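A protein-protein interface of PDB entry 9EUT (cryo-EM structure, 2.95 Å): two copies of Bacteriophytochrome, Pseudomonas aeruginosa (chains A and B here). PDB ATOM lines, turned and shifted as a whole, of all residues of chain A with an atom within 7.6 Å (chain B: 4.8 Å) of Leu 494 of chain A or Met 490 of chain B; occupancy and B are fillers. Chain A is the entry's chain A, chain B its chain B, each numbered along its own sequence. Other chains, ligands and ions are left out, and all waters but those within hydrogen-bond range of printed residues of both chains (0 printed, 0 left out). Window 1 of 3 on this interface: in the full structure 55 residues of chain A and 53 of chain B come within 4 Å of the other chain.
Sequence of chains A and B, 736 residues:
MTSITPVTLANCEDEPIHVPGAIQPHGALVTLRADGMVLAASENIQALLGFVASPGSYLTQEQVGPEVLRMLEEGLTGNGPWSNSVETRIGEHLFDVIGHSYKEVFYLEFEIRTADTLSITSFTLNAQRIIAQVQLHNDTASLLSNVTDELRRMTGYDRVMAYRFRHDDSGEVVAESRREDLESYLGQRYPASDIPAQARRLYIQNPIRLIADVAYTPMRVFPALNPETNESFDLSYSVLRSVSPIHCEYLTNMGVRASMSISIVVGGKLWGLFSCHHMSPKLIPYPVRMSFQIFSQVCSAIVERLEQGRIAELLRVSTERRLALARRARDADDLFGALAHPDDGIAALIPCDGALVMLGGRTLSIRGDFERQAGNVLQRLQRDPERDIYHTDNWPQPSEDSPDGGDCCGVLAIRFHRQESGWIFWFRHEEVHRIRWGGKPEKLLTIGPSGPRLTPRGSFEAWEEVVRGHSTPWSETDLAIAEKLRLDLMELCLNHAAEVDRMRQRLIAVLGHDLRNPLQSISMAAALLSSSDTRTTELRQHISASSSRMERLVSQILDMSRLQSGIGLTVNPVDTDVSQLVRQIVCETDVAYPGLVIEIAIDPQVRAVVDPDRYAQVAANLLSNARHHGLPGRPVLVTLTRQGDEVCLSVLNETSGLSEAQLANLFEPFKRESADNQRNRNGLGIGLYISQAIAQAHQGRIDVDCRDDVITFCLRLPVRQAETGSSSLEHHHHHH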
ATOM      1  N   PHE A 416     -20.574  20.950  13.926  1.00  0.00           N
ATOM      2  CA  PHE A 416     -21.193  20.224  15.022  1.00  0.00           C
ATOM      3  C   PHE A 416     -20.337  20.162  16.285  1.00  0.00           C
ATOM      4  O   PHE A 416     -20.850  19.771  17.334  1.00  0.00           O
ATOM      5  CB  PHE A 416     -21.614  18.815  14.560  1.00  0.00           C
ATOM      6  CG  PHE A 416     -20.479  17.901  14.186  1.00  0.00           C
ATOM      7  CD1 PHE A 416     -19.656  17.345  15.134  1.00  0.00           C
ATOM      8  CD2 PHE A 416     -20.304  17.527  12.878  1.00  0.00           C
ATOM      9  CE1 PHE A 416     -18.639  16.496  14.770  1.00  0.00           C
ATOM     10  CE2 PHE A 416     -19.300  16.670  12.523  1.00  0.00           C
ATOM     11  CZ  PHE A 416     -18.465  16.160  13.464  1.00  0.00           C
ATOM     12  N   HIS A 417     -19.057  20.513  16.223  1.00  0.00           N
ATOM     13  CA  HIS A 417     -18.222  20.515  17.427  1.00  0.00           C
ATOM     14  C   HIS A 417     -17.246  21.679  17.244  1.00  0.00           C
ATOM     15  O   HIS A 417     -16.137  21.500  16.737  1.00  0.00           O
ATOM     16  CB  HIS A 417     -17.510  19.185  17.612  1.00  0.00           C
ATOM     17  CG  HIS A 417     -16.904  19.000  18.969  1.00  0.00           C
ATOM     18  ND1 HIS A 417     -16.385  20.042  19.707  1.00  0.00           N
ATOM     19  CD2 HIS A 417     -16.737  17.887  19.722  1.00  0.00           C
ATOM     20  CE1 HIS A 417     -15.927  19.579  20.857  1.00  0.00           C
ATOM     21  NE2 HIS A 417     -16.126  18.274  20.888  1.00  0.00           N
ATOM     22  N   LEU A 487     -27.567  19.603  14.811  1.00  0.00           N
ATOM     23  CA  LEU A 487     -28.014  19.477  16.197  1.00  0.00           C
ATOM     24  C   LEU A 487     -27.914  18.041  16.712  1.00  0.00           C
ATOM     25  O   LEU A 487     -27.469  17.821  17.845  1.00  0.00           O
ATOM     26  CB  LEU A 487     -29.438  20.006  16.334  1.00  0.00           C
ATOM     27  CG  LEU A 487     -29.549  21.491  16.002  1.00  0.00           C
ATOM     28  CD1 LEU A 487     -30.991  21.897  15.788  1.00  0.00           C
ATOM     29  CD2 LEU A 487     -28.909  22.311  17.099  1.00  0.00           C
ATOM     30  N   ASP A 488     -28.338  17.054  15.915  1.00  0.00           N
ATOM     31  CA  ASP A 488     -28.221  15.654  16.327  1.00  0.00           C
ATOM     32  C   ASP A 488     -26.773  15.263  16.606  1.00  0.00           C
ATOM     33  O   ASP A 488     -26.479  14.584  17.600  1.00  0.00           O
ATOM     34  CB  ASP A 488     -28.807  14.750  15.247  1.00  0.00           C
ATOM     35  CG  ASP A 488     -30.319  14.754  15.239  1.00  0.00           C
ATOM     36  OD1 ASP A 488     -30.919  15.352  16.156  1.00  0.00           O
ATOM     37  OD2 ASP A 488     -30.911  14.151  14.318  1.00  0.00           O
ATOM     38  N   LEU A 489     -25.847  15.751  15.786  1.00  0.00           N
ATOM     39  CA  LEU A 489     -24.435  15.462  15.985  1.00  0.00           C
ATOM     40  C   LEU A 489     -23.861  16.243  17.152  1.00  0.00           C
ATOM     41  O   LEU A 489     -22.965  15.748  17.832  1.00  0.00           O
ATOM     42  CB  LEU A 489     -23.664  15.726  14.696  1.00  0.00           C
ATOM     43  CG  LEU A 489     -23.967  14.646  13.664  1.00  0.00           C
ATOM     44  CD1 LEU A 489     -23.329  14.952  12.364  1.00  0.00           C
ATOM     45  CD2 LEU A 489     -23.423  13.342  14.185  1.00  0.00           C
ATOM     46  N   MET A 490     -24.329  17.466  17.393  1.00  0.00           N
ATOM     47  CA  MET A 490     -23.866  18.192  18.571  1.00  0.00           C
ATOM     48  C   MET A 490     -24.273  17.453  19.834  1.00  0.00           C
ATOM     49  O   MET A 490     -23.480  17.302  20.765  1.00  0.00           O
ATOM     50  CB  MET A 490     -24.449  19.602  18.594  1.00  0.00           C
ATOM     51  CG  MET A 490     -23.649  20.664  17.890  1.00  0.00           C
ATOM     52  SD  MET A 490     -24.673  22.102  17.563  1.00  0.00           S
ATOM     53  CE  MET A 490     -25.584  22.188  19.102  1.00  0.00           C
ATOM     54  N   GLU A 491     -25.529  17.011  19.891  1.00  0.00           N
ATOM     55  CA  GLU A 491     -26.012  16.245  21.036  1.00  0.00           C
ATOM     56  C   GLU A 491     -25.204  14.967  21.243  1.00  0.00           C
ATOM     57  O   GLU A 491     -24.794  14.653  22.369  1.00  0.00           O
ATOM     58  CB  GLU A 491     -27.490  15.925  20.845  1.00  0.00           C
ATOM     59  CG  GLU A 491     -28.132  15.206  21.998  1.00  0.00           C
ATOM     60  CD  GLU A 491     -29.642  15.304  21.954  1.00  0.00           C
ATOM     61  OE1 GLU A 491     -30.220  15.091  20.868  1.00  0.00           O
ATOM     62  OE2 GLU A 491     -30.255  15.588  23.002  1.00  0.00           O
ATOM     63  N   LEU A 492     -24.921  14.244  20.157  1.00  0.00           N
ATOM     64  CA  LEU A 492     -24.106  13.037  20.268  1.00  0.00           C
ATOM     65  C   LEU A 492     -22.669  13.349  20.664  1.00  0.00           C
ATOM     66  O   LEU A 492     -22.057  12.592  21.421  1.00  0.00           O
ATOM     67  CB  LEU A 492     -24.142  12.268  18.951  1.00  0.00           C
ATOM     68  CG  LEU A 492     -23.303  10.997  18.870  1.00  0.00           C
ATOM     69  CD1 LEU A 492     -23.682  10.026  19.963  1.00  0.00           C
ATOM     70  CD2 LEU A 492     -23.492  10.364  17.515  1.00  0.00           C
ATOM     71  N   CYS A 493     -22.103  14.440  20.150  1.00  0.00           N
ATOM     72  CA  CYS A 493     -20.744  14.824  20.512  1.00  0.00           C
ATOM     73  C   CYS A 493     -20.654  15.239  21.973  1.00  0.00           C
ATOM     74  O   CYS A 493     -19.641  14.990  22.634  1.00  0.00           O
ATOM     75  CB  CYS A 493     -20.259  15.952  19.605  1.00  0.00           C
ATOM     76  SG  CYS A 493     -19.869  15.431  17.926  1.00  0.00           S
ATOM     77  N   LEU A 494     -21.702  15.876  22.491  1.00  0.00           N
ATOM     78  CA  LEU A 494     -21.729  16.239  23.901  1.00  0.00           C
ATOM     79  C   LEU A 494     -21.811  14.996  24.774  1.00  0.00           C
ATOM     80  O   LEU A 494     -21.091  14.877  25.770  1.00  0.00           O
ATOM     81  CB  LEU A 494     -22.899  17.177  24.177  1.00  0.00           C
ATOM     82  CG  LEU A 494     -23.099  17.607  25.628  1.00  0.00           C
ATOM     83  CD1 LEU A 494     -21.845  18.257  26.164  1.00  0.00           C
ATOM     84  CD2 LEU A 494     -24.277  18.553  25.738  1.00  0.00           C
ATOM     85  N   ASN A 495     -22.688  14.057  24.417  1.00  0.00           N
ATOM     86  CA  ASN A 495     -22.779  12.817  25.182  1.00  0.00           C
ATOM     87  C   ASN A 495     -21.467  12.039  25.123  1.00  0.00           C
ATOM     88  O   ASN A 495     -21.033  11.449  26.120  1.00  0.00           O
ATOM     89  CB  ASN A 495     -23.931  11.968  24.657  1.00  0.00           C
ATOM     90  CG  ASN A 495     -25.275  12.623  24.870  1.00  0.00           C
ATOM     91  OD1 ASN A 495     -25.364  13.704  25.450  1.00  0.00           O
ATOM     92  ND2 ASN A 495     -26.332  11.969  24.405  1.00  0.00           N
ATOM     93  N   HIS A 496     -20.827  12.030  23.955  1.00  0.00           N
ATOM     94  CA  HIS A 496     -19.532  11.380  23.766  1.00  0.00           C
ATOM     95  C   HIS A 496     -18.411  12.078  24.531  1.00  0.00           C
ATOM     96  O   HIS A 496     -17.637  11.428  25.243  1.00  0.00           O
ATOM     97  CB  HIS A 496     -19.201  11.330  22.273  1.00  0.00           C
ATOM     98  CG  HIS A 496     -17.783  10.956  21.981  1.00  0.00           C
ATOM     99  ND1 HIS A 496     -17.300   9.675  22.142  1.00  0.00           N
ATOM    100  CD2 HIS A 496     -16.738  11.700  21.548  1.00  0.00           C
ATOM    101  CE1 HIS A 496     -16.020   9.645  21.816  1.00  0.00           C
ATOM    102  NE2 HIS A 496     -15.655  10.861  21.452  1.00  0.00           N
ATOM    103  N   ALA A 497     -18.303  13.401  24.388  1.00  0.00           N
ATOM    104  CA  ALA A 497     -17.209  14.146  25.011  1.00  0.00           C
ATOM    105  C   ALA A 497     -17.339  14.243  26.527  1.00  0.00           C
ATOM    106  O   ALA A 497     -16.324  14.348  27.222  1.00  0.00           O
ATOM    107  CB  ALA A 497     -17.116  15.546  24.408  1.00  0.00           C
ATOM    108  N   ALA A 498     -18.558  14.220  27.060  1.00  0.00           N
ATOM    109  CA  ALA A 498     -18.729  14.327  28.506  1.00  0.00           C
ATOM    110  C   ALA A 498     -18.125  13.154  29.271  1.00  0.00           C
ATOM    111  O   ALA A 498     -17.879  13.280  30.476  1.00  0.00           O
ATOM    112  CB  ALA A 498     -20.211  14.461  28.842  1.00  0.00           C
ATOM    113  N   GLU A 499     -17.882  12.019  28.612  1.00  0.00           N
ATOM    114  CA  GLU A 499     -17.251  10.883  29.282  1.00  0.00           C
ATOM    115  C   GLU A 499     -15.819  11.187  29.709  1.00  0.00           C
ATOM    116  O   GLU A 499     -15.334  10.615  30.692  1.00  0.00           O
ATOM    117  CB  GLU A 499     -17.284   9.651  28.375  1.00  0.00           C
ATOM    118  CG  GLU A 499     -16.681   8.393  28.996  1.00  0.00           C
ATOM    119  CD  GLU A 499     -17.376   7.951  30.273  1.00  0.00           C
ATOM    120  OE1 GLU A 499     -18.533   8.359  30.513  1.00  0.00           O
ATOM    121  OE2 GLU A 499     -16.754   7.196  31.049  1.00  0.00           O
ATOM    122  N   VAL A 500     -15.139  12.084  28.997  1.00  0.00           N
ATOM    123  CA  VAL A 500     -13.765  12.451  29.335  1.00  0.00           C
ATOM    124  C   VAL A 500     -13.674  12.978  30.763  1.00  0.00           C
ATOM    125  O   VAL A 500     -12.703  12.705  31.482  1.00  0.00           O
ATOM    126  CB  VAL A 500     -13.235  13.484  28.322  1.00  0.00           C
ATOM    127  CG1 VAL A 500     -11.800  13.874  28.647  1.00  0.00           C
ATOM    128  CG2 VAL A 500     -13.346  12.948  26.901  1.00  0.00           C
ATOM    129  N   ASP B 388     -35.641  13.322  27.971  1.00  0.00           N
ATOM    130  CA  ASP B 388     -35.059  14.652  28.083  1.00  0.00           C
ATOM    131  C   ASP B 388     -36.089  15.767  28.226  1.00  0.00           C
ATOM    132  O   ASP B 388     -35.699  16.904  28.501  1.00  0.00           O
ATOM    133  CB  ASP B 388     -34.162  14.954  26.872  1.00  0.00           C
ATOM    134  CG  ASP B 388     -32.822  14.234  26.935  1.00  0.00           C
ATOM    135  OD1 ASP B 388     -32.312  14.012  28.053  1.00  0.00           O
ATOM    136  OD2 ASP B 388     -32.269  13.904  25.866  1.00  0.00           O
ATOM    137  N   ARG B 415     -34.149  18.742  29.760  1.00  0.00           N
ATOM    138  CA  ARG B 415     -32.768  18.436  30.110  1.00  0.00           C
ATOM    139  C   ARG B 415     -31.841  18.907  29.005  1.00  0.00           C
ATOM    140  O   ARG B 415     -31.947  18.456  27.862  1.00  0.00           O
ATOM    141  CB  ARG B 415     -32.576  16.943  30.344  1.00  0.00           C
ATOM    142  CG  ARG B 415     -31.194  16.574  30.845  1.00  0.00           C
ATOM    143  CD  ARG B 415     -31.206  15.187  31.451  1.00  0.00           C
ATOM    144  NE  ARG B 415     -31.544  14.156  30.479  1.00  0.00           N
ATOM    145  CZ  ARG B 415     -31.776  12.890  30.792  1.00  0.00           C
ATOM    146  NH1 ARG B 415     -31.644  12.449  32.032  1.00  0.00           N
ATOM    147  NH2 ARG B 415     -32.139  12.041  29.837  1.00  0.00           N
ATOM    148  N   PHE B 416     -30.920  19.791  29.360  1.00  0.00           N
ATOM    149  CA  PHE B 416     -29.973  20.382  28.432  1.00  0.00           C
ATOM    150  C   PHE B 416     -28.532  19.944  28.674  1.00  0.00           C
ATOM    151  O   PHE B 416     -27.632  20.423  27.986  1.00  0.00           O
ATOM    152  CB  PHE B 416     -30.111  21.908  28.465  1.00  0.00           C
ATOM    153  CG  PHE B 416     -29.731  22.524  29.770  1.00  0.00           C
ATOM    154  CD1 PHE B 416     -28.441  22.913  30.026  1.00  0.00           C
ATOM    155  CD2 PHE B 416     -30.686  22.733  30.738  1.00  0.00           C
ATOM    156  CE1 PHE B 416     -28.103  23.484  31.229  1.00  0.00           C
ATOM    157  CE2 PHE B 416     -30.356  23.305  31.936  1.00  0.00           C
ATOM    158  CZ  PHE B 416     -29.060  23.684  32.182  1.00  0.00           C
ATOM    159  N   HIS B 417     -28.284  19.078  29.654  1.00  0.00           N
ATOM    160  CA  HIS B 417     -26.936  18.557  29.884  1.00  0.00           C
ATOM    161  C   HIS B 417     -27.137  17.273  30.697  1.00  0.00           C
ATOM    162  O   HIS B 417     -27.205  17.309  31.924  1.00  0.00           O
ATOM    163  CB  HIS B 417     -26.056  19.558  30.597  1.00  0.00           C
ATOM    164  CG  HIS B 417     -24.601  19.227  30.543  1.00  0.00           C
ATOM    165  ND1 HIS B 417     -24.131  17.940  30.400  1.00  0.00           N
ATOM    166  CD2 HIS B 417     -23.507  20.023  30.585  1.00  0.00           C
ATOM    167  CE1 HIS B 417     -22.810  17.956  30.371  1.00  0.00           C
ATOM    168  NE2 HIS B 417     -22.406  19.208  30.481  1.00  0.00           N
ATOM    169  N   LEU B 485     -35.369  25.640  23.157  1.00  0.00           N
ATOM    170  CA  LEU B 485     -34.442  26.140  24.159  1.00  0.00           C
ATOM    171  C   LEU B 485     -33.528  25.028  24.643  1.00  0.00           C
ATOM    172  O   LEU B 485     -32.369  25.280  24.988  1.00  0.00           O
ATOM    173  CB  LEU B 485     -35.211  26.758  25.325  1.00  0.00           C
ATOM    174  CG  LEU B 485     -34.346  27.400  26.403  1.00  0.00           C
ATOM    175  CD1 LEU B 485     -33.778  28.707  25.896  1.00  0.00           C
ATOM    176  CD2 LEU B 485     -35.142  27.634  27.652  1.00  0.00           C
ATOM    177  N   ARG B 486     -34.047  23.799  24.740  1.00  0.00           N
ATOM    178  CA  ARG B 486     -33.214  22.682  25.169  1.00  0.00           C
ATOM    179  C   ARG B 486     -31.965  22.581  24.313  1.00  0.00           C
ATOM    180  O   ARG B 486     -30.858  22.385  24.825  1.00  0.00           O
ATOM    181  CB  ARG B 486     -34.007  21.387  25.090  1.00  0.00           C
ATOM    182  CG  ARG B 486     -33.395  20.256  25.856  1.00  0.00           C
ATOM    183  CD  ARG B 486     -34.233  19.008  25.717  1.00  0.00           C
ATOM    184  NE  ARG B 486     -34.030  18.356  24.433  1.00  0.00           N
ATOM    185  CZ  ARG B 486     -33.004  17.566  24.162  1.00  0.00           C
ATOM    186  NH1 ARG B 486     -32.042  17.358  25.044  1.00  0.00           N
ATOM    187  NH2 ARG B 486     -32.934  16.978  22.972  1.00  0.00           N
ATOM    188  N   LEU B 487     -32.127  22.762  23.001  1.00  0.00           N
ATOM    189  CA  LEU B 487     -31.012  22.698  22.062  1.00  0.00           C
ATOM    190  C   LEU B 487     -30.120  23.924  22.180  1.00  0.00           C
ATOM    191  O   LEU B 487     -28.887  23.812  22.149  1.00  0.00           O
ATOM    192  CB  LEU B 487     -31.549  22.560  20.641  1.00  0.00           C
ATOM    193  CG  LEU B 487     -32.525  21.401  20.439  1.00  0.00           C
ATOM    194  CD1 LEU B 487     -33.040  21.364  19.016  1.00  0.00           C
ATOM    195  CD2 LEU B 487     -31.879  20.077  20.813  1.00  0.00           C
ATOM    196  N   ASP B 488     -30.728  25.104  22.314  1.00  0.00           N
ATOM    197  CA  ASP B 488     -29.937  26.319  22.476  1.00  0.00           C
ATOM    198  C   ASP B 488     -29.072  26.275  23.727  1.00  0.00           C
ATOM    199  O   ASP B 488     -28.017  26.916  23.770  1.00  0.00           O
ATOM    200  CB  ASP B 488     -30.843  27.545  22.513  1.00  0.00           C
ATOM    201  CG  ASP B 488     -31.614  27.729  21.234  1.00  0.00           C
ATOM    202  OD1 ASP B 488     -31.289  27.047  20.242  1.00  0.00           O
ATOM    203  OD2 ASP B 488     -32.527  28.578  21.211  1.00  0.00           O
ATOM    204  N   LEU B 489     -29.506  25.560  24.757  1.00  0.00           N
ATOM    205  CA  LEU B 489     -28.720  25.410  25.977  1.00  0.00           C
ATOM    206  C   LEU B 489     -27.766  24.225  25.926  1.00  0.00           C
ATOM    207  O   LEU B 489     -26.709  24.262  26.568  1.00  0.00           O
ATOM    208  CB  LEU B 489     -29.651  25.311  27.183  1.00  0.00           C
ATOM    209  CG  LEU B 489     -30.428  26.616  27.296  1.00  0.00           C
ATOM    210  CD1 LEU B 489     -31.326  26.607  28.459  1.00  0.00           C
ATOM    211  CD2 LEU B 489     -29.448  27.750  27.448  1.00  0.00           C
ATOM    212  N   MET B 490     -28.084  23.198  25.138  1.00  0.00           N
ATOM    213  CA  MET B 490     -27.141  22.102  24.958  1.00  0.00           C
ATOM    214  C   MET B 490     -25.921  22.579  24.185  1.00  0.00           C
ATOM    215  O   MET B 490     -24.793  22.165  24.473  1.00  0.00           O
ATOM    216  CB  MET B 490     -27.814  20.946  24.222  1.00  0.00           C
ATOM    217  CG  MET B 490     -28.348  19.848  25.107  1.00  0.00           C
ATOM    218  SD  MET B 490     -28.869  18.405  24.169  1.00  0.00           S
ATOM    219  CE  MET B 490     -28.788  17.148  25.437  1.00  0.00           C
ATOM    220  N   GLU B 491     -26.133  23.455  23.206  1.00  0.00           N
ATOM    221  CA  GLU B 491     -25.021  24.044  22.466  1.00  0.00           C
ATOM    222  C   GLU B 491     -24.058  24.763  23.405  1.00  0.00           C
ATOM    223  O   GLU B 491     -22.844  24.519  23.387  1.00  0.00           O
ATOM    224  CB  GLU B 491     -25.566  25.014  21.419  1.00  0.00           C
ATOM    225  CG  GLU B 491     -24.522  25.906  20.770  1.00  0.00           C
ATOM    226  CD  GLU B 491     -23.923  25.313  19.517  1.00  0.00           C
ATOM    227  OE1 GLU B 491     -24.666  25.154  18.528  1.00  0.00           O
ATOM    228  OE2 GLU B 491     -22.711  25.018  19.513  1.00  0.00           O
ATOM    229  N   LEU B 492     -24.592  25.680  24.212  1.00  0.00           N
ATOM    230  CA  LEU B 492     -23.789  26.445  25.161  1.00  0.00           C
ATOM    231  C   LEU B 492     -23.096  25.549  26.177  1.00  0.00           C
ATOM    232  O   LEU B 492     -21.933  25.785  26.521  1.00  0.00           O
ATOM    233  CB  LEU B 492     -24.665  27.485  25.860  1.00  0.00           C
ATOM    234  CG  LEU B 492     -24.818  28.854  25.186  1.00  0.00           C
ATOM    235  CD1 LEU B 492     -25.006  28.749  23.685  1.00  0.00           C
ATOM    236  CD2 LEU B 492     -25.996  29.581  25.792  1.00  0.00           C
ATOM    237  N   CYS B 493     -23.769  24.500  26.647  1.00  0.00           N
ATOM    238  CA  CYS B 493     -23.114  23.582  27.574  1.00  0.00           C
ATOM    239  C   CYS B 493     -21.955  22.841  26.918  1.00  0.00           C
ATOM    240  O   CYS B 493     -20.904  22.666  27.537  1.00  0.00           O
ATOM    241  CB  CYS B 493     -24.125  22.601  28.148  1.00  0.00           C
ATOM    242  SG  CYS B 493     -25.272  23.388  29.260  1.00  0.00           S
ATOM    243  N   LEU B 494     -22.121  22.385  25.677  1.00  0.00           N
ATOM    244  CA  LEU B 494     -21.022  21.706  24.996  1.00  0.00           C
ATOM    245  C   LEU B 494     -19.835  22.646  24.808  1.00  0.00           C
ATOM    246  O   LEU B 494     -18.695  22.323  25.187  1.00  0.00           O
ATOM    247  CB  LEU B 494     -21.503  21.164  23.649  1.00  0.00           C
ATOM    248  CG  LEU B 494     -20.482  20.589  22.666  1.00  0.00           C
ATOM    249  CD1 LEU B 494     -19.760  19.385  23.245  1.00  0.00           C
ATOM    250  CD2 LEU B 494     -21.155  20.237  21.355  1.00  0.00           C
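The side-chain carboxylate (OE2) of Glu 491 of chain A lies within salt-bridge range of the guanidinium group (NH2) of Arg 486 of chain B (3.0 Å).
SD of Met 490 of chain A sits close to OE1 of Glu 491 of chain B, at 3.2 Å.
OE2 of Glu 491 of chain A lies close to SD of Met 490 of chain B.
The guanidinium group of Arg 415 of chain B lies within salt-bridge range of the side-chain carboxylate of Asp 388 of chain B (2.5 Å).
OD1 of Asn 495 of chain A sits close to O of Glu 491 of chain A (3.3 Å).
NH1 of Arg 486 of chain B lies within salt-bridge range of OD2 of Asp 388 of chain B (3.6 Å).
The guanidinium group (NH1) of Arg 486 of chain B lies within hydrogen-bond range of the backbone carbonyl oxygen (O) of Arg 415 of chain B (3.0 Å).
The guanidinium group (NH1) of Arg 486 of chain B lies close to the side-chain sulfur (SD) of Met 490 of chain B, 3.5 Å away.
Leu 487 of chain A touches Leu 487 of chain B.
Met 490 of chain A touches Leu 494 of chain B.
Glu 491 of chain A touches Asp 388 of chain B (OE2 to OD2, 3.9 Å).
CD2 of Leu 494 of chain A touches O of Met 490 of chain B, 3.9 Å away.
CD1 of Leu 494 of chain A touches CA of Leu 494 of chain B, 3.7 Å away.
Of the printed residues of chain B, Met 490 of chain A touches Glu 491 and Leu 494.
Of the printed residues of chain B, Glu 491 of chain A touches Asp 388, Arg 486 and Met 490.
Leu 494 of chain A touches just these residues of chain B: Met 490 and Leu 494.
Printed residues of chain A within 4 Å of Asp 388 of chain B: Glu 491 (3.9 Å).
His 417 of chain B touches none of the printed residues of chain A.
Of chain A, only Glu 491 (3.2 Å) and Leu 494 (3.9 Å) come within 4 Å of Met 490 of chain B.
The nearest residue of chain B that does not touch Leu 494 of chain A is His 417 of chain B (4.3 Å).
The nearest residue of chain A that does not touch Met 490 of chain B is Asn 495 of chain A (4.9 Å).
The nearest printed residue of chain A that does not touch Leu 487 of chain B is Met 490 of chain A (4.8 Å).
Printed residues of chain B that touch a printed residue of chain A: Asp 388, Arg 486, Leu 487, Met 490, Glu 491 and Leu 494.
Of the 16 printed residues of chain A, 4 touch a printed residue of chain B.
Printed residues of chain A that touch a printed residue of chain B: Leu 487, Met 490, Glu 491 and Leu 494.
Among the printed residues, 8 pairs touch across the chains.
Leu 487 of chain A touches its own counterpart, Leu 487 of chain B.
Met 490 of chain A touches Glu 491 of chain B, and with the chains exchanged Glu 491 of chain A touches Met 490 of chain B.
Met 490 of chain A touches Leu 494 of chain B, and with the chains exchanged Leu 494 of chain A touches Met 490 of chain B.
Leu 494 of chain A touches its own counterpart, Leu 494 of chain B.
Positions printed for both chains: 416, 417, 487, 488, 489, 490, 491, 492, 493 and 494.
Of the 8 pairs that touch across the chains among the printed residues, 6 have their exchanged pair printed and touching as well.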
